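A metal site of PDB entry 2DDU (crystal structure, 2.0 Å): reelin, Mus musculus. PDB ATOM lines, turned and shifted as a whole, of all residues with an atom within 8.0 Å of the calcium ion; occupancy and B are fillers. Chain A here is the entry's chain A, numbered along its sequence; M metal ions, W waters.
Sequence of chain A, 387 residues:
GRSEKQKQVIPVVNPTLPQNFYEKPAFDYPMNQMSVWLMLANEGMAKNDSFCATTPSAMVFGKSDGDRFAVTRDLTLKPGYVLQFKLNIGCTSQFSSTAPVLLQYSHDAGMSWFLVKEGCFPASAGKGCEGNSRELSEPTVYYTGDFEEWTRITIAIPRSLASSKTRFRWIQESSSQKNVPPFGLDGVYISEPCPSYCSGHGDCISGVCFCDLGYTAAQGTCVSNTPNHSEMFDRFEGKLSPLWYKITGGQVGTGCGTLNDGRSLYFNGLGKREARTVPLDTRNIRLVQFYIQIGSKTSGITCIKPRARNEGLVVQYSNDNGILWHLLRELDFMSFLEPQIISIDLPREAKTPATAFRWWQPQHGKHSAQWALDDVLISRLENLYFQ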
ATOM      1  N   ASP A 234     -16.828  -7.475  -6.002  1.00  0.00           N
ATOM      2  CA  ASP A 234     -15.532  -7.645  -5.352  1.00  0.00           C
ATOM      3  C   ASP A 234     -15.558  -6.875  -4.046  1.00  0.00           C
ATOM      4  O   ASP A 234     -15.802  -5.668  -4.022  1.00  0.00           O
ATOM      5  CB  ASP A 234     -14.403  -7.153  -6.267  1.00  0.00           C
ATOM      6  CG  ASP A 234     -13.038  -7.758  -5.925  1.00  0.00           C
ATOM      7  OD1 ASP A 234     -12.819  -8.203  -4.790  1.00  0.00           O
ATOM      8  OD2 ASP A 234     -12.175  -7.766  -6.805  1.00  0.00           O
ATOM      9  N   ARG A 235     -15.313  -7.601  -2.947  1.00  0.00           N
ATOM     10  CA  ARG A 235     -15.221  -7.025  -1.610  1.00  0.00           C
ATOM     11  C   ARG A 235     -13.781  -6.686  -1.180  1.00  0.00           C
ATOM     12  O   ARG A 235     -13.564  -6.086  -0.125  1.00  0.00           O
ATOM     13  CB  ARG A 235     -15.869  -7.956  -0.581  1.00  0.00           C
ATOM     14  CG  ARG A 235     -17.340  -8.149  -0.798  1.00  0.00           C
ATOM     15  CD  ARG A 235     -17.967  -9.141   0.193  1.00  0.00           C
ATOM     16  NE  ARG A 235     -17.483  -8.992   1.559  1.00  0.00           N
ATOM     17  CZ  ARG A 235     -17.905  -8.077   2.431  1.00  0.00           C
ATOM     18  NH1 ARG A 235     -18.838  -7.178   2.111  1.00  0.00           N
ATOM     19  NH2 ARG A 235     -17.365  -8.048   3.650  1.00  0.00           N
ATOM     20  N   PHE A 236     -12.820  -7.098  -1.986  1.00  0.00           N
ATOM     21  CA  PHE A 236     -11.406  -6.747  -1.806  1.00  0.00           C
ATOM     22  C   PHE A 236     -10.802  -7.308  -0.509  1.00  0.00           C
ATOM     23  O   PHE A 236     -10.053  -6.622   0.187  1.00  0.00           O
ATOM     24  CB  PHE A 236     -11.216  -5.222  -1.907  1.00  0.00           C
ATOM     25  CG  PHE A 236     -11.752  -4.646  -3.190  1.00  0.00           C
ATOM     26  CD1 PHE A 236     -12.737  -3.676  -3.182  1.00  0.00           C
ATOM     27  CD2 PHE A 236     -11.290  -5.118  -4.428  1.00  0.00           C
ATOM     28  CE1 PHE A 236     -13.246  -3.158  -4.385  1.00  0.00           C
ATOM     29  CE2 PHE A 236     -11.783  -4.606  -5.629  1.00  0.00           C
ATOM     30  CZ  PHE A 236     -12.769  -3.619  -5.597  1.00  0.00           C
ATOM     31  N   GLU A 237     -11.151  -8.559  -0.219  1.00  0.00           N
ATOM     32  CA  GLU A 237     -10.688  -9.218   1.007  1.00  0.00           C
ATOM     33  C   GLU A 237      -9.468 -10.094   0.785  1.00  0.00           C
ATOM     34  O   GLU A 237      -8.800 -10.471   1.741  1.00  0.00           O
ATOM     35  CB  GLU A 237     -11.831 -10.006   1.659  1.00  0.00           C
ATOM     36  CG  GLU A 237     -13.025  -9.141   2.130  1.00  0.00           C
ATOM     37  CD  GLU A 237     -12.612  -7.886   2.915  1.00  0.00           C
ATOM     38  OE1 GLU A 237     -11.543  -7.874   3.572  1.00  0.00           O
ATOM     39  OE2 GLU A 237     -13.387  -6.899   2.886  1.00  0.00           O
ATOM     40  N   GLY A 238      -9.174 -10.386  -0.473  1.00  0.00           N
ATOM     41  CA  GLY A 238      -8.016 -11.209  -0.810  1.00  0.00           C
ATOM     42  C   GLY A 238      -7.710 -11.131  -2.278  1.00  0.00           C
ATOM     43  O   GLY A 238      -7.286 -10.069  -2.777  1.00  0.00           O
ATOM     44  N   VAL A 252      -5.007  -4.432  -3.167  1.00  0.00           N
ATOM     45  CA  VAL A 252      -5.784  -4.640  -1.966  1.00  0.00           C
ATOM     46  C   VAL A 252      -4.971  -4.063  -0.800  1.00  0.00           C
ATOM     47  O   VAL A 252      -3.776  -4.306  -0.712  1.00  0.00           O
ATOM     48  CB  VAL A 252      -6.126  -6.153  -1.784  1.00  0.00           C
ATOM     49  CG1 VAL A 252      -6.768  -6.383  -0.420  1.00  0.00           C
ATOM     50  CG2 VAL A 252      -7.082  -6.615  -2.913  1.00  0.00           C
ATOM     51  N   GLY A 253      -5.613  -3.262   0.044  1.00  0.00           N
ATOM     52  CA  GLY A 253      -4.927  -2.581   1.137  1.00  0.00           C
ATOM     53  C   GLY A 253      -5.875  -1.839   2.061  1.00  0.00           C
ATOM     54  O   GLY A 253      -7.084  -2.022   2.004  1.00  0.00           O
ATOM     55  N   THR A 258     -10.937   1.935   6.881  1.00  0.00           N
ATOM     56  CA  THR A 258     -12.079   1.118   6.521  1.00  0.00           C
ATOM     57  C   THR A 258     -13.073   1.925   5.685  1.00  0.00           C
ATOM     58  O   THR A 258     -13.408   3.059   6.030  1.00  0.00           O
ATOM     59  CB  THR A 258     -12.725   0.543   7.809  1.00  0.00           C
ATOM     60  OG1 THR A 258     -11.736  -0.211   8.500  1.00  0.00           O
ATOM     61  CG2 THR A 258     -13.908  -0.354   7.492  1.00  0.00           C
ATOM     62  N   LEU A 259     -13.527   1.347   4.575  1.00  0.00           N
ATOM     63  CA  LEU A 259     -14.601   1.971   3.787  1.00  0.00           C
ATOM     64  C   LEU A 259     -15.971   1.367   4.154  1.00  0.00           C
ATOM     65  O   LEU A 259     -16.750   1.983   4.890  1.00  0.00           O
ATOM     66  CB  LEU A 259     -14.299   1.895   2.288  1.00  0.00           C
ATOM     67  CG  LEU A 259     -13.462   3.029   1.672  1.00  0.00           C
ATOM     68  CD1 LEU A 259     -12.054   3.228   2.346  1.00  0.00           C
ATOM     69  CD2 LEU A 259     -13.330   2.798   0.160  1.00  0.00           C
ATOM     70  N   ASN A 260     -16.286   0.189   3.641  1.00  0.00           N
ATOM     71  CA  ASN A 260     -17.462  -0.541   4.131  1.00  0.00           C
ATOM     72  C   ASN A 260     -16.996  -1.540   5.203  1.00  0.00           C
ATOM     73  O   ASN A 260     -17.282  -1.380   6.385  1.00  0.00           O
ATOM     74  CB  ASN A 260     -18.238  -1.250   3.003  1.00  0.00           C
ATOM     75  CG  ASN A 260     -19.523  -1.907   3.519  1.00  0.00           C
ATOM     76  OD1 ASN A 260     -20.148  -1.417   4.444  1.00  0.00           O
ATOM     77  ND2 ASN A 260     -19.915  -3.005   2.900  1.00  0.00           N
ATOM     78  N   ASP A 261     -16.246  -2.547   4.787  1.00  0.00           N
ATOM     79  CA  ASP A 261     -15.613  -3.417   5.765  1.00  0.00           C
ATOM     80  C   ASP A 261     -14.392  -4.107   5.222  1.00  0.00           C
ATOM     81  O   ASP A 261     -14.229  -4.270   3.991  1.00  0.00           O
ATOM     82  CB  ASP A 261     -16.612  -4.392   6.380  1.00  0.00           C
ATOM     83  CG  ASP A 261     -17.382  -5.177   5.348  1.00  0.00           C
ATOM     84  OD1 ASP A 261     -18.635  -5.169   5.402  1.00  0.00           O
ATOM     85  OD2 ASP A 261     -16.746  -5.810   4.492  1.00  0.00           O
ATOM     86  N   GLY A 262     -13.511  -4.469   6.164  1.00  0.00           N
ATOM     87  CA  GLY A 262     -12.271  -5.162   5.864  1.00  0.00           C
ATOM     88  C   GLY A 262     -11.350  -4.326   5.013  1.00  0.00           C
ATOM     89  O   GLY A 262     -11.269  -3.110   5.176  1.00  0.00           O
ATOM     90  N   ARG A 263     -10.656  -4.997   4.093  1.00  0.00           N
ATOM     91  CA  ARG A 263      -9.708  -4.365   3.191  1.00  0.00           C
ATOM     92  C   ARG A 263     -10.428  -3.740   1.962  1.00  0.00           C
ATOM     93  O   ARG A 263     -11.597  -4.008   1.720  1.00  0.00           O
ATOM     94  CB  ARG A 263      -8.629  -5.375   2.789  1.00  0.00           C
ATOM     95  CG  ARG A 263      -7.943  -6.009   4.019  1.00  0.00           C
ATOM     96  CD  ARG A 263      -6.550  -6.496   3.718  1.00  0.00           C
ATOM     97  NE  ARG A 263      -6.528  -7.808   3.070  1.00  0.00           N
ATOM     98  CZ  ARG A 263      -5.480  -8.291   2.388  1.00  0.00           C
ATOM     99  NH1 ARG A 263      -4.383  -7.552   2.245  1.00  0.00           N
ATOM    100  NH2 ARG A 263      -5.539  -9.494   1.844  1.00  0.00           N
ATOM    101  N   SER A 264      -9.713  -2.892   1.241  1.00  0.00           N
ATOM    102  CA  SER A 264     -10.309  -2.158   0.118  1.00  0.00           C
ATOM    103  C   SER A 264      -9.339  -2.270  -1.064  1.00  0.00           C
ATOM    104  O   SER A 264      -8.242  -2.780  -0.891  1.00  0.00           O
ATOM    105  CB  SER A 264     -10.518  -0.708   0.516  1.00  0.00           C
ATOM    106  OG  SER A 264      -9.268  -0.094   0.817  1.00  0.00           O
ATOM    107  N   LEU A 265      -9.756  -1.825  -2.245  1.00  0.00           N
ATOM    108  CA  LEU A 265      -8.844  -1.620  -3.346  1.00  0.00           C
ATOM    109  C   LEU A 265      -8.253  -0.206  -3.224  1.00  0.00           C
ATOM    110  O   LEU A 265      -8.942   0.795  -3.470  1.00  0.00           O
ATOM    111  CB  LEU A 265      -9.579  -1.783  -4.695  1.00  0.00           C
ATOM    112  CG  LEU A 265      -8.714  -1.845  -5.965  1.00  0.00           C
ATOM    113  CD1 LEU A 265      -7.642  -2.921  -5.884  1.00  0.00           C
ATOM    114  CD2 LEU A 265      -9.593  -2.050  -7.213  1.00  0.00           C
ATOM    115  N   TYR A 291     -18.372   1.626  -2.854  1.00  0.00           N
ATOM    116  CA  TYR A 291     -17.992   2.642  -1.859  1.00  0.00           C
ATOM    117  C   TYR A 291     -16.731   3.351  -2.347  1.00  0.00           C
ATOM    118  O   TYR A 291     -15.920   2.752  -3.009  1.00  0.00           O
ATOM    119  CB  TYR A 291     -17.703   1.981  -0.501  1.00  0.00           C
ATOM    120  CG  TYR A 291     -18.952   1.478   0.219  1.00  0.00           C
ATOM    121  CD1 TYR A 291     -19.599   0.315  -0.197  1.00  0.00           C
ATOM    122  CD2 TYR A 291     -19.468   2.158   1.307  1.00  0.00           C
ATOM    123  CE1 TYR A 291     -20.747  -0.151   0.451  1.00  0.00           C
ATOM    124  CE2 TYR A 291     -20.622   1.697   1.984  1.00  0.00           C
ATOM    125  CZ  TYR A 291     -21.244   0.545   1.537  1.00  0.00           C
ATOM    126  OH  TYR A 291     -22.372   0.082   2.197  1.00  0.00           O
ATOM    127  N   LEU A 373     -11.604   2.004  -3.240  1.00  0.00           N
ATOM    128  CA  LEU A 373     -12.950   1.510  -3.525  1.00  0.00           C
ATOM    129  C   LEU A 373     -13.252   0.355  -2.574  1.00  0.00           C
ATOM    130  O   LEU A 373     -12.323  -0.322  -2.074  1.00  0.00           O
ATOM    131  CB  LEU A 373     -13.033   0.996  -4.980  1.00  0.00           C
ATOM    132  CG  LEU A 373     -12.680   1.983  -6.110  1.00  0.00           C
ATOM    133  CD1 LEU A 373     -12.540   1.282  -7.472  1.00  0.00           C
ATOM    134  CD2 LEU A 373     -13.707   3.097  -6.161  1.00  0.00           C
ATOM    135  N   ASP A 374     -14.533   0.105  -2.313  1.00  0.00           N
ATOM    136  CA  ASP A 374     -14.929  -1.122  -1.587  1.00  0.00           C
ATOM    137  C   ASP A 374     -16.212  -1.631  -2.208  1.00  0.00           C
ATOM    138  O   ASP A 374     -16.985  -0.849  -2.795  1.00  0.00           O
ATOM    139  CB  ASP A 374     -15.133  -0.843  -0.099  1.00  0.00           C
ATOM    140  CG  ASP A 374     -14.841  -2.086   0.781  1.00  0.00           C
ATOM    141  OD1 ASP A 374     -14.558  -3.159   0.229  1.00  0.00           O
ATOM    142  OD2 ASP A 374     -14.881  -1.957   2.025  1.00  0.00           O
ATOM    143  N   ASP A 375     -16.425  -2.953  -2.107  1.00  0.00           N
ATOM    144  CA  ASP A 375     -17.685  -3.576  -2.572  1.00  0.00           C
ATOM    145  C   ASP A 375     -18.177  -3.072  -3.920  1.00  0.00           C
ATOM    146  O   ASP A 375     -19.291  -2.543  -4.034  1.00  0.00           O
ATOM    147  CB  ASP A 375     -18.799  -3.416  -1.533  1.00  0.00           C
ATOM    148  CG  ASP A 375     -18.546  -4.228  -0.268  1.00  0.00           C
ATOM    149  OD1 ASP A 375     -17.535  -4.952  -0.201  1.00  0.00           O
ATOM    150  OD2 ASP A 375     -19.357  -4.111   0.671  1.00  0.00           O
ATOM    151  N   VAL A 376     -17.355  -3.236  -4.939  1.00  0.00           N
ATOM    152  CA  VAL A 376     -17.745  -2.931  -6.318  1.00  0.00           C
ATOM    153  C   VAL A 376     -18.739  -4.001  -6.763  1.00  0.00           C
ATOM    154  O   VAL A 376     -18.430  -5.208  -6.748  1.00  0.00           O
ATOM    155  CB  VAL A 376     -16.538  -2.906  -7.255  1.00  0.00           C
ATOM    156  CG1 VAL A 376     -16.998  -2.834  -8.727  1.00  0.00           C
ATOM    157  CG2 VAL A 376     -15.639  -1.709  -6.916  1.00  0.00           C
HETATM  158 CA    CA M   1     -13.885  -4.859   1.779  1.00  0.00          CA
HETATM  159  O   HOH W   1     -16.030  -5.457   1.990  1.00  0.00           O
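The guanidinium group (NH1) of Arg 235 lies within salt-bridge range of the side-chain carboxylate (OD2) of Asp 375, 3.4 Å away.
The side-chain carboxylate of Asp 374 is in hydrogen-bond range of the backbone NH of Asn 260 (3.0 Å).
The backbone carbonyl oxygen (O) of Asp 374 is in hydrogen-bond range of the backbone NH (N) of Tyr 291, 2.8 Å away.
Within 4 Å of the calcium ion: Arg 235, Glu 237, Asp 261, Arg 263 and Asp 374.
The calcium ion is bound by water W1, the backbone carbonyl oxygen (O) of Arg 235, the backbone carbonyl oxygen (O) of Asp 261, the side-chain carboxylate (OE2) of Glu 237, the side-chain carboxylate (OD1) of Asp 374 and the backbone carbonyl oxygen (O) of Arg 263.
The calcium ion has six donor atoms within binding distance.
Slightly farther from the calcium ion lies the side-chain carboxylate (OD2) of Asp 374 (3.1 Å).
Water W1 lies within hydrogen-bond range of OD2 of Asp 261 (2.6 Å), OD1 of Asp 375 (2.7 Å) and NH1 of Arg 235 (3.3 Å).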
